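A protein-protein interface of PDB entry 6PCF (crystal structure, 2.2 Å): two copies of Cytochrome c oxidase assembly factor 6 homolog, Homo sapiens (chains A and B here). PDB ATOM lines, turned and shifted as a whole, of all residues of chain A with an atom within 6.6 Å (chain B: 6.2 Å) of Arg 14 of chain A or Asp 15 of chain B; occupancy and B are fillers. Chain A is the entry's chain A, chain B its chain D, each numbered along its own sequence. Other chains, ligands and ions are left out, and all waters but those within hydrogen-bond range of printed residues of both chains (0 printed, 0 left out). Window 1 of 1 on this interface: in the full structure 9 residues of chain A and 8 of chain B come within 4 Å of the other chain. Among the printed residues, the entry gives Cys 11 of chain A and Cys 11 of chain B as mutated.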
ATOM      1  N   VAL A   9      18.748  -2.109 -22.955  1.00  0.00           N
ATOM      2  CA  VAL A   9      18.675  -0.967 -21.993  1.00  0.00           C
ATOM      3  C   VAL A   9      17.198  -0.685 -21.685  1.00  0.00           C
ATOM      4  O   VAL A   9      16.394  -0.613 -22.629  1.00  0.00           O
ATOM      5  CB  VAL A   9      19.395   0.280 -22.542  1.00  0.00           C
ATOM      6  CG1 VAL A   9      19.088   1.528 -21.726  1.00  0.00           C
ATOM      7  CG2 VAL A   9      20.896   0.052 -22.623  1.00  0.00           C
ATOM      8  N   CYS A  10      16.853  -0.535 -20.405  1.00  0.00           N
ATOM      9  CA  CYS A  10      15.449  -0.406 -19.931  1.00  0.00           C
ATOM     10  C   CYS A  10      14.729   0.669 -20.751  1.00  0.00           C
ATOM     11  O   CYS A  10      13.638   0.377 -21.249  1.00  0.00           O
ATOM     12  CB  CYS A  10      15.397  -0.090 -18.438  1.00  0.00           C
ATOM     13  SG  CYS A  10      13.786   0.514 -17.866  1.00  0.00           S
ATOM     14  N   CYS A  11      15.326   1.855 -20.911  1.00  0.00           N
ATOM     15  CA  CYS A  11      14.661   3.029 -21.544  1.00  0.00           C
ATOM     16  C   CYS A  11      14.561   2.856 -23.065  1.00  0.00           C
ATOM     17  O   CYS A  11      13.596   3.397 -23.655  1.00  0.00           O
ATOM     18  CB  CYS A  11      15.361   4.327 -21.159  1.00  0.00           C
ATOM     19  SG  CYS A  11      14.844   4.910 -19.523  1.00  0.00           S
ATOM     20  N   GLY A  12      15.500   2.130 -23.679  1.00  0.00           N
ATOM     21  CA  GLY A  12      15.425   1.720 -25.095  1.00  0.00           C
ATOM     22  C   GLY A  12      14.194   0.867 -25.365  1.00  0.00           C
ATOM     23  O   GLY A  12      13.460   1.170 -26.322  1.00  0.00           O
ATOM     24  N   ALA A  13      13.959  -0.162 -24.546  1.00  0.00           N
ATOM     25  CA  ALA A  13      12.803  -1.080 -24.684  1.00  0.00           C
ATOM     26  C   ALA A  13      11.509  -0.308 -24.391  1.00  0.00           C
ATOM     27  O   ALA A  13      10.495  -0.526 -25.075  1.00  0.00           O
ATOM     28  CB  ALA A  13      12.974  -2.280 -23.786  1.00  0.00           C
ATOM     29  N   ARG A  14      11.543   0.607 -23.432  1.00  0.00           N
ATOM     30  CA  ARG A  14      10.372   1.459 -23.096  1.00  0.00           C
ATOM     31  C   ARG A  14      10.029   2.346 -24.306  1.00  0.00           C
ATOM     32  O   ARG A  14       8.847   2.405 -24.682  1.00  0.00           O
ATOM     33  CB  ARG A  14      10.700   2.273 -21.843  1.00  0.00           C
ATOM     34  CG  ARG A  14       9.624   3.267 -21.442  1.00  0.00           C
ATOM     35  CD  ARG A  14      10.244   4.346 -20.583  1.00  0.00           C
ATOM     36  NE  ARG A  14      11.037   5.252 -21.390  1.00  0.00           N
ATOM     37  CZ  ARG A  14      11.614   6.354 -20.934  1.00  0.00           C
ATOM     38  NH1 ARG A  14      11.493   6.680 -19.659  1.00  0.00           N
ATOM     39  NH2 ARG A  14      12.301   7.129 -21.755  1.00  0.00           N
ATOM     40  N   ASP A  15      11.031   3.010 -24.890  1.00  0.00           N
ATOM     41  CA  ASP A  15      10.878   3.936 -26.049  1.00  0.00           C
ATOM     42  C   ASP A  15      10.328   3.189 -27.273  1.00  0.00           C
ATOM     43  O   ASP A  15       9.505   3.797 -27.992  1.00  0.00           O
ATOM     44  CB  ASP A  15      12.197   4.649 -26.372  1.00  0.00           C
ATOM     45  CG  ASP A  15      12.584   5.695 -25.335  1.00  0.00           C
ATOM     46  OD1 ASP A  15      11.760   5.960 -24.434  1.00  0.00           O
ATOM     47  OD2 ASP A  15      13.708   6.221 -25.424  1.00  0.00           O
ATOM     48  N   GLU A  16      10.739   1.931 -27.492  1.00  0.00           N
ATOM     49  CA  GLU A  16      10.290   1.091 -28.640  1.00  0.00           C
ATOM     50  C   GLU A  16       8.827   0.695 -28.417  1.00  0.00           C
ATOM     51  O   GLU A  16       8.050   0.745 -29.380  1.00  0.00           O
ATOM     52  CB  GLU A  16      11.154  -0.164 -28.822  1.00  0.00           C
ATOM     53  CG  GLU A  16      12.274  -0.012 -29.842  1.00  0.00           C
ATOM     54  CD  GLU A  16      12.766  -1.311 -30.469  1.00  0.00           C
ATOM     55  OE1 GLU A  16      13.480  -1.239 -31.492  1.00  0.00           O
ATOM     56  OE2 GLU A  16      12.437  -2.394 -29.940  1.00  0.00           O
ATOM     57  N   TYR A  17       8.469   0.312 -27.191  1.00  0.00           N
ATOM     58  CA  TYR A  17       7.068   0.022 -26.798  1.00  0.00           C
ATOM     59  C   TYR A  17       6.220   1.278 -27.030  1.00  0.00           C
ATOM     60  O   TYR A  17       5.140   1.170 -27.626  1.00  0.00           O
ATOM     61  CB  TYR A  17       6.983  -0.460 -25.348  1.00  0.00           C
ATOM     62  CG  TYR A  17       5.573  -0.571 -24.827  1.00  0.00           C
ATOM     63  CD1 TYR A  17       4.680  -1.462 -25.397  1.00  0.00           C
ATOM     64  CD2 TYR A  17       5.122   0.225 -23.782  1.00  0.00           C
ATOM     65  CE1 TYR A  17       3.379  -1.578 -24.933  1.00  0.00           C
ATOM     66  CE2 TYR A  17       3.821   0.129 -23.314  1.00  0.00           C
ATOM     67  CZ  TYR A  17       2.946  -0.779 -23.891  1.00  0.00           C
ATOM     68  OH  TYR A  17       1.662  -0.904 -23.447  1.00  0.00           O
ATOM     69  N   TRP A  18       6.703   2.439 -26.580  1.00  0.00           N
ATOM     70  CA  TRP A  18       5.981   3.737 -26.697  1.00  0.00           C
ATOM     71  C   TRP A  18       5.891   4.172 -28.167  1.00  0.00           C
ATOM     72  O   TRP A  18       4.862   4.776 -28.528  1.00  0.00           O
ATOM     73  CB  TRP A  18       6.643   4.820 -25.835  1.00  0.00           C
ATOM     74  CG  TRP A  18       6.376   4.714 -24.366  1.00  0.00           C
ATOM     75  CD1 TRP A  18       5.515   3.870 -23.724  1.00  0.00           C
ATOM     76  CD2 TRP A  18       6.969   5.533 -23.345  1.00  0.00           C
ATOM     77  NE1 TRP A  18       5.547   4.095 -22.374  1.00  0.00           N
ATOM     78  CE2 TRP A  18       6.429   5.113 -22.112  1.00  0.00           C
ATOM     79  CE3 TRP A  18       7.917   6.563 -23.354  1.00  0.00           C
ATOM     80  CZ2 TRP A  18       6.797   5.705 -20.904  1.00  0.00           C
ATOM     81  CZ3 TRP A  18       8.280   7.148 -22.161  1.00  0.00           C
ATOM     82  CH2 TRP A  18       7.725   6.721 -20.953  1.00  0.00           C
ATOM     83  N   LYS A  19       6.920   3.897 -28.980  1.00  0.00           N
ATOM     84  CA  LYS A  19       6.902   4.193 -30.439  1.00  0.00           C
ATOM     85  C   LYS A  19       5.767   3.393 -31.088  1.00  0.00           C
ATOM     86  O   LYS A  19       5.009   3.988 -31.871  1.00  0.00           O
ATOM     87  CB  LYS A  19       8.246   3.880 -31.100  1.00  0.00           C
ATOM     88  N   LEU A  34       6.501  -6.067 -27.841  1.00  0.00           N
ATOM     89  CA  LEU A  34       7.444  -5.057 -27.300  1.00  0.00           C
ATOM     90  C   LEU A  34       7.102  -4.739 -25.836  1.00  0.00           C
ATOM     91  O   LEU A  34       8.010  -4.287 -25.123  1.00  0.00           O
ATOM     92  CB  LEU A  34       7.383  -3.814 -28.192  1.00  0.00           C
ATOM     93  CG  LEU A  34       7.954  -4.007 -29.597  1.00  0.00           C
ATOM     94  CD1 LEU A  34       7.444  -2.933 -30.544  1.00  0.00           C
ATOM     95  CD2 LEU A  34       9.477  -4.022 -29.570  1.00  0.00           C
ATOM     96  N   SER A  37       9.181  -7.317 -23.956  1.00  0.00           N
ATOM     97  CA  SER A  37      10.614  -6.897 -23.942  1.00  0.00           C
ATOM     98  C   SER A  37      10.811  -5.736 -22.957  1.00  0.00           C
ATOM     99  O   SER A  37      11.861  -5.706 -22.286  1.00  0.00           O
ATOM    100  CB  SER A  37      11.112  -6.538 -25.325  1.00  0.00           C
ATOM    101  OG  SER A  37      10.961  -7.638 -26.212  1.00  0.00           O
ATOM    102  N   PHE A  38       9.845  -4.810 -22.894  1.00  0.00           N
ATOM    103  CA  PHE A  38       9.779  -3.691 -21.916  1.00  0.00           C
ATOM    104  C   PHE A  38       9.789  -4.279 -20.495  1.00  0.00           C
ATOM    105  O   PHE A  38      10.687  -3.941 -19.690  1.00  0.00           O
ATOM    106  CB  PHE A  38       8.558  -2.812 -22.218  1.00  0.00           C
ATOM    107  CG  PHE A  38       8.281  -1.681 -21.254  1.00  0.00           C
ATOM    108  CD1 PHE A  38       9.305  -1.045 -20.569  1.00  0.00           C
ATOM    109  CD2 PHE A  38       6.983  -1.231 -21.058  1.00  0.00           C
ATOM    110  CE1 PHE A  38       9.033  -0.004 -19.688  1.00  0.00           C
ATOM    111  CE2 PHE A  38       6.713  -0.186 -20.187  1.00  0.00           C
ATOM    112  CZ  PHE A  38       7.738   0.427 -19.505  1.00  0.00           C
ATOM    113  N   SER A  41      13.111  -5.880 -19.616  1.00  0.00           N
ATOM    114  CA  SER A  41      14.248  -4.924 -19.584  1.00  0.00           C
ATOM    115  C   SER A  41      14.222  -4.045 -18.327  1.00  0.00           C
ATOM    116  O   SER A  41      15.295  -3.524 -17.977  1.00  0.00           O
ATOM    117  CB  SER A  41      14.256  -4.060 -20.820  1.00  0.00           C
ATOM    118  OG  SER A  41      14.404  -4.837 -21.993  1.00  0.00           O
ATOM    119  N   CYS A  42      13.051  -3.844 -17.706  1.00  0.00           N
ATOM    120  CA  CYS A  42      12.814  -2.799 -16.668  1.00  0.00           C
ATOM    121  C   CYS A  42      12.266  -3.406 -15.382  1.00  0.00           C
ATOM    122  O   CYS A  42      11.307  -4.176 -15.419  1.00  0.00           O
ATOM    123  CB  CYS A  42      11.828  -1.741 -17.152  1.00  0.00           C
ATOM    124  SG  CYS A  42      12.409  -0.827 -18.603  1.00  0.00           S
ATOM    125  N   TYR A  49       5.969   3.638 -12.594  1.00  0.00           N
ATOM    126  CA  TYR A  49       6.248   5.075 -12.826  1.00  0.00           C
ATOM    127  C   TYR A  49       6.047   5.387 -14.323  1.00  0.00           C
ATOM    128  O   TYR A  49       5.192   6.234 -14.656  1.00  0.00           O
ATOM    129  CB  TYR A  49       7.642   5.466 -12.319  1.00  0.00           C
ATOM    130  CG  TYR A  49       8.101   6.767 -12.925  1.00  0.00           C
ATOM    131  CD1 TYR A  49       7.339   7.916 -12.773  1.00  0.00           C
ATOM    132  CD2 TYR A  49       9.231   6.837 -13.726  1.00  0.00           C
ATOM    133  CE1 TYR A  49       7.709   9.114 -13.362  1.00  0.00           C
ATOM    134  CE2 TYR A  49       9.620   8.030 -14.317  1.00  0.00           C
ATOM    135  CZ  TYR A  49       8.854   9.172 -14.137  1.00  0.00           C
ATOM    136  OH  TYR A  49       9.220  10.352 -14.714  1.00  0.00           O
ATOM    137  N   PHE A  50       6.772   4.705 -15.215  1.00  0.00           N
ATOM    138  CA  PHE A  50       6.763   4.990 -16.679  1.00  0.00           C
ATOM    139  C   PHE A  50       5.334   4.912 -17.242  1.00  0.00           C
ATOM    140  O   PHE A  50       5.010   5.726 -18.136  1.00  0.00           O
ATOM    141  CB  PHE A  50       7.687   4.053 -17.472  1.00  0.00           C
ATOM    142  CG  PHE A  50       9.161   4.136 -17.151  1.00  0.00           C
ATOM    143  CD1 PHE A  50       9.775   5.346 -16.862  1.00  0.00           C
ATOM    144  CD2 PHE A  50       9.948   2.993 -17.169  1.00  0.00           C
ATOM    145  CE1 PHE A  50      11.130   5.406 -16.567  1.00  0.00           C
ATOM    146  CE2 PHE A  50      11.301   3.055 -16.875  1.00  0.00           C
ATOM    147  CZ  PHE A  50      11.893   4.262 -16.577  1.00  0.00           C
ATOM    148  N   ARG A  53       3.566   8.099 -16.132  1.00  0.00           N
ATOM    149  CA  ARG A  53       4.125   9.221 -16.941  1.00  0.00           C
ATOM    150  C   ARG A  53       3.457   9.251 -18.321  1.00  0.00           C
ATOM    151  O   ARG A  53       3.007  10.330 -18.745  1.00  0.00           O
ATOM    152  CB  ARG A  53       5.641   9.096 -17.096  1.00  0.00           C
ATOM    153  CG  ARG A  53       6.272  10.205 -17.927  1.00  0.00           C
ATOM    154  CD  ARG A  53       7.783  10.091 -17.982  1.00  0.00           C
ATOM    155  NE  ARG A  53       8.420  11.325 -18.434  1.00  0.00           N
ATOM    156  CZ  ARG A  53       8.661  11.665 -19.703  1.00  0.00           C
ATOM    157  NH1 ARG A  53       8.327  10.867 -20.707  1.00  0.00           N
ATOM    158  NH2 ARG A  53       9.248  12.821 -19.962  1.00  0.00           N
ATOM    159  N   CYS B  10      20.874   8.880 -16.447  1.00  0.00           N
ATOM    160  CA  CYS B  10      21.008   9.453 -17.811  1.00  0.00           C
ATOM    161  C   CYS B  10      19.625   9.556 -18.465  1.00  0.00           C
ATOM    162  O   CYS B  10      19.268  10.653 -18.934  1.00  0.00           O
ATOM    163  CB  CYS B  10      21.962   8.628 -18.665  1.00  0.00           C
ATOM    164  SG  CYS B  10      21.997   9.153 -20.397  1.00  0.00           S
ATOM    165  N   CYS B  11      18.858   8.470 -18.453  1.00  0.00           N
ATOM    166  CA  CYS B  11      17.498   8.401 -19.058  1.00  0.00           C
ATOM    167  C   CYS B  11      16.565   9.429 -18.402  1.00  0.00           C
ATOM    168  O   CYS B  11      15.906  10.187 -19.142  1.00  0.00           O
ATOM    169  CB  CYS B  11      16.894   7.012 -18.918  1.00  0.00           C
ATOM    170  SG  CYS B  11      15.208   6.916 -19.570  1.00  0.00           S
ATOM    171  N   GLY B  12      16.509   9.459 -17.068  1.00  0.00           N
ATOM    172  CA  GLY B  12      15.720  10.455 -16.314  1.00  0.00           C
ATOM    173  C   GLY B  12      16.028  11.869 -16.780  1.00  0.00           C
ATOM    174  O   GLY B  12      15.086  12.595 -17.144  1.00  0.00           O
ATOM    175  N   ALA B  13      17.307  12.248 -16.779  1.00  0.00           N
ATOM    176  CA  ALA B  13      17.792  13.582 -17.200  1.00  0.00           C
ATOM    177  C   ALA B  13      17.402  13.851 -18.666  1.00  0.00           C
ATOM    178  O   ALA B  13      17.063  15.009 -18.991  1.00  0.00           O
ATOM    179  CB  ALA B  13      19.284  13.670 -16.975  1.00  0.00           C
ATOM    180  N   ARG B  14      17.416  12.827 -19.523  1.00  0.00           N
ATOM    181  CA  ARG B  14      16.995  12.933 -20.952  1.00  0.00           C
ATOM    182  C   ARG B  14      15.475  13.139 -21.043  1.00  0.00           C
ATOM    183  O   ARG B  14      15.044  13.989 -21.849  1.00  0.00           O
ATOM    184  CB  ARG B  14      17.411  11.687 -21.740  1.00  0.00           C
ATOM    185  CG  ARG B  14      17.264  11.825 -23.250  1.00  0.00           C
ATOM    186  CD  ARG B  14      16.116  11.002 -23.801  1.00  0.00           C
ATOM    187  NE  ARG B  14      16.307   9.579 -23.549  1.00  0.00           N
ATOM    188  CZ  ARG B  14      15.487   8.615 -23.956  1.00  0.00           C
ATOM    189  NH1 ARG B  14      14.405   8.910 -24.658  1.00  0.00           N
ATOM    190  NH2 ARG B  14      15.761   7.351 -23.673  1.00  0.00           N
ATOM    191  N   ASP B  15      14.704  12.382 -20.258  1.00  0.00           N
ATOM    192  CA  ASP B  15      13.219  12.471 -20.173  1.00  0.00           C
ATOM    193  C   ASP B  15      12.815  13.915 -19.855  1.00  0.00           C
ATOM    194  O   ASP B  15      12.014  14.472 -20.625  1.00  0.00           O
ATOM    195  CB  ASP B  15      12.653  11.492 -19.137  1.00  0.00           C
ATOM    196  CG  ASP B  15      12.729  10.034 -19.574  1.00  0.00           C
ATOM    197  OD1 ASP B  15      13.102   9.793 -20.743  1.00  0.00           O
ATOM    198  OD2 ASP B  15      12.426   9.144 -18.745  1.00  0.00           O
ATOM    199  N   GLU B  16      13.361  14.494 -18.781  1.00  0.00           N
ATOM    200  CA  GLU B  16      13.038  15.877 -18.330  1.00  0.00           C
ATOM    201  C   GLU B  16      13.405  16.873 -19.440  1.00  0.00           C
ATOM    202  O   GLU B  16      12.561  17.729 -19.781  1.00  0.00           O
ATOM    203  CB  GLU B  16      13.764  16.211 -17.024  1.00  0.00           C
ATOM    204  CG  GLU B  16      12.955  15.901 -15.780  1.00  0.00           C
ATOM    205  CD  GLU B  16      13.295  16.776 -14.588  1.00  0.00           C
ATOM    206  OE1 GLU B  16      14.493  17.057 -14.386  1.00  0.00           O
ATOM    207  OE2 GLU B  16      12.358  17.191 -13.876  1.00  0.00           O
ATOM    208  N   TYR B  17      14.611  16.755 -19.998  1.00  0.00           N
ATOM    209  CA  TYR B  17      15.122  17.645 -21.076  1.00  0.00           C
ATOM    210  C   TYR B  17      14.164  17.575 -22.274  1.00  0.00           C
ATOM    211  O   TYR B  17      13.653  18.623 -22.681  1.00  0.00           O
ATOM    212  CB  TYR B  17      16.568  17.292 -21.436  1.00  0.00           C
ATOM    213  CG  TYR B  17      17.107  17.994 -22.658  1.00  0.00           C
ATOM    214  CD1 TYR B  17      17.044  19.375 -22.778  1.00  0.00           C
ATOM    215  CD2 TYR B  17      17.683  17.281 -23.698  1.00  0.00           C
ATOM    216  CE1 TYR B  17      17.537  20.029 -23.899  1.00  0.00           C
ATOM    217  CE2 TYR B  17      18.179  17.918 -24.825  1.00  0.00           C
ATOM    218  CZ  TYR B  17      18.109  19.296 -24.925  1.00  0.00           C
ATOM    219  OH  TYR B  17      18.597  19.923 -26.034  1.00  0.00           O
ATOM    220  N   TRP B  18      13.908  16.380 -22.814  1.00  0.00           N
ATOM    221  CA  TRP B  18      13.029  16.202 -24.001  1.00  0.00           C
ATOM    222  C   TRP B  18      11.615  16.728 -23.698  1.00  0.00           C
ATOM    223  O   TRP B  18      11.029  17.357 -24.593  1.00  0.00           O
ATOM    224  CB  TRP B  18      13.031  14.746 -24.475  1.00  0.00           C
ATOM    225  CG  TRP B  18      14.196  14.387 -25.348  1.00  0.00           C
ATOM    226  CD1 TRP B  18      15.362  15.080 -25.519  1.00  0.00           C
ATOM    227  CD2 TRP B  18      14.316  13.207 -26.162  1.00  0.00           C
ATOM    228  NE1 TRP B  18      16.183  14.425 -26.401  1.00  0.00           N
ATOM    229  CE2 TRP B  18      15.574  13.267 -26.801  1.00  0.00           C
ATOM    230  CE3 TRP B  18      13.484  12.113 -26.416  1.00  0.00           C
ATOM    231  CZ2 TRP B  18      16.016  12.269 -27.667  1.00  0.00           C
ATOM    232  CZ3 TRP B  18      13.918  11.132 -27.283  1.00  0.00           C
ATOM    233  CH2 TRP B  18      15.168  11.211 -27.898  1.00  0.00           C
ATOM    234  N   LYS B  19      11.101  16.519 -22.480  1.00  0.00           N
ATOM    235  CA  LYS B  19       9.762  17.010 -22.035  1.00  0.00           C
ATOM    236  C   LYS B  19       9.705  18.538 -22.181  1.00  0.00           C
ATOM    237  O   LYS B  19       8.781  19.030 -22.859  1.00  0.00           O
ATOM    238  CB  LYS B  19       9.477  16.567 -20.594  1.00  0.00           C
ATOM    239  CG  LYS B  19       8.167  17.072 -19.995  1.00  0.00           C
ATOM    240  CD  LYS B  19       7.705  16.269 -18.797  1.00  0.00           C
ATOM    241  CE  LYS B  19       6.448  16.817 -18.155  1.00  0.00           C
ATOM    242  NZ  LYS B  19       6.647  18.205 -17.674  1.00  0.00           N
ATOM    243  N   CYS B  20      10.659  19.251 -21.574  1.00  0.00           N
ATOM    244  CA  CYS B  20      10.856  20.721 -21.709  1.00  0.00           C
ATOM    245  C   CYS B  20      10.794  21.134 -23.189  1.00  0.00           C
ATOM    246  O   CYS B  20      10.032  22.068 -23.502  1.00  0.00           O
ATOM    247  CB  CYS B  20      12.181  21.148 -21.082  1.00  0.00           C
ATOM    248  SG  CYS B  20      12.453  22.941 -21.072  1.00  0.00           S
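The side-chain sulfur (SG) of Cys 11 of chain B is disulfide-bonded to the side-chain sulfur (SG) of Cys 11 of chain A, 2.0 Å away. SG of Cys 11 of chain B is in hydrogen-bond range of NH2 of Arg 14 of chain A (3.6 Å). The guanidinium group (NH1) of Arg 14 of chain A is in salt-bridge range of the side-chain carboxylate (OD2) of Asp 15 of chain B, at 2.8 Å. The side-chain carboxylate (OD2) of Asp 15 of chain A is in salt-bridge range of the guanidinium group (NH1) of Arg 14 of chain B, 2.9 Å away. The guanidinium group (NH2) of Arg 53 of chain A is in hydrogen-bond range of the backbone carbonyl oxygen (O) of Asp 15 of chain B (3.3 Å).
NH1 of Arg 14 of chain A sits at hydrogen-bond distance from SG of Cys 11 of chain A, at 3.8 Å. NH2 of Arg 14 of chain A lies within salt-bridge range of OD1 of Asp 15 of chain A (3.0 Å). The side-chain sulfur of Cys 10 of chain A forms a disulfide with the side-chain sulfur of Cys 42 of chain A, at 2.1 Å.
Among the printed residues, pairs that only touch across the chains: Cys 11 of chain A with Arg 14 of chain B (3.95 Å), Arg 14 of chain A with Arg 14 of chain B (3.96 Å) and Arg 53 of chain A with Lys 19 of chain B (3.8 Å).
Of chain B, only Cys 11, Arg 14 and Asp 15 come within 4 Å of Arg 14 of chain A. Asp 15 of chain B touches two residues of chain A. Of the printed residues of chain B, Asp 15 of chain A touches Arg 14 (2.9 Å). Of the printed residues of chain A, Lys 19 of chain B touches Arg 53. The nearest printed residue of chain B that does not touch Arg 14 of chain A is Gly 12 of chain B (6.3 Å). The nearest printed residue of chain B that does not touch Asp 15 of chain A is Trp 18 of chain B (5.3 Å).
Printed residues of chain A that touch a printed residue of chain B: Cys 11, Arg 14, Asp 15 and Arg 53. Among the printed residues, 8 pairs touch across the chains.
Cys 11 of chain A touches its own counterpart, Cys 11 of chain B. Cys 11 of chain A touches Arg 14 of chain B, and with the chains exchanged Arg 14 of chain A touches Cys 11 of chain B. Arg 14 of chain B touches its own counterpart, Arg 14 of chain A. Arg 14 of chain A touches Asp 15 of chain B, and with the chains exchanged Asp 15 of chain A touches Arg 14 of chain B.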
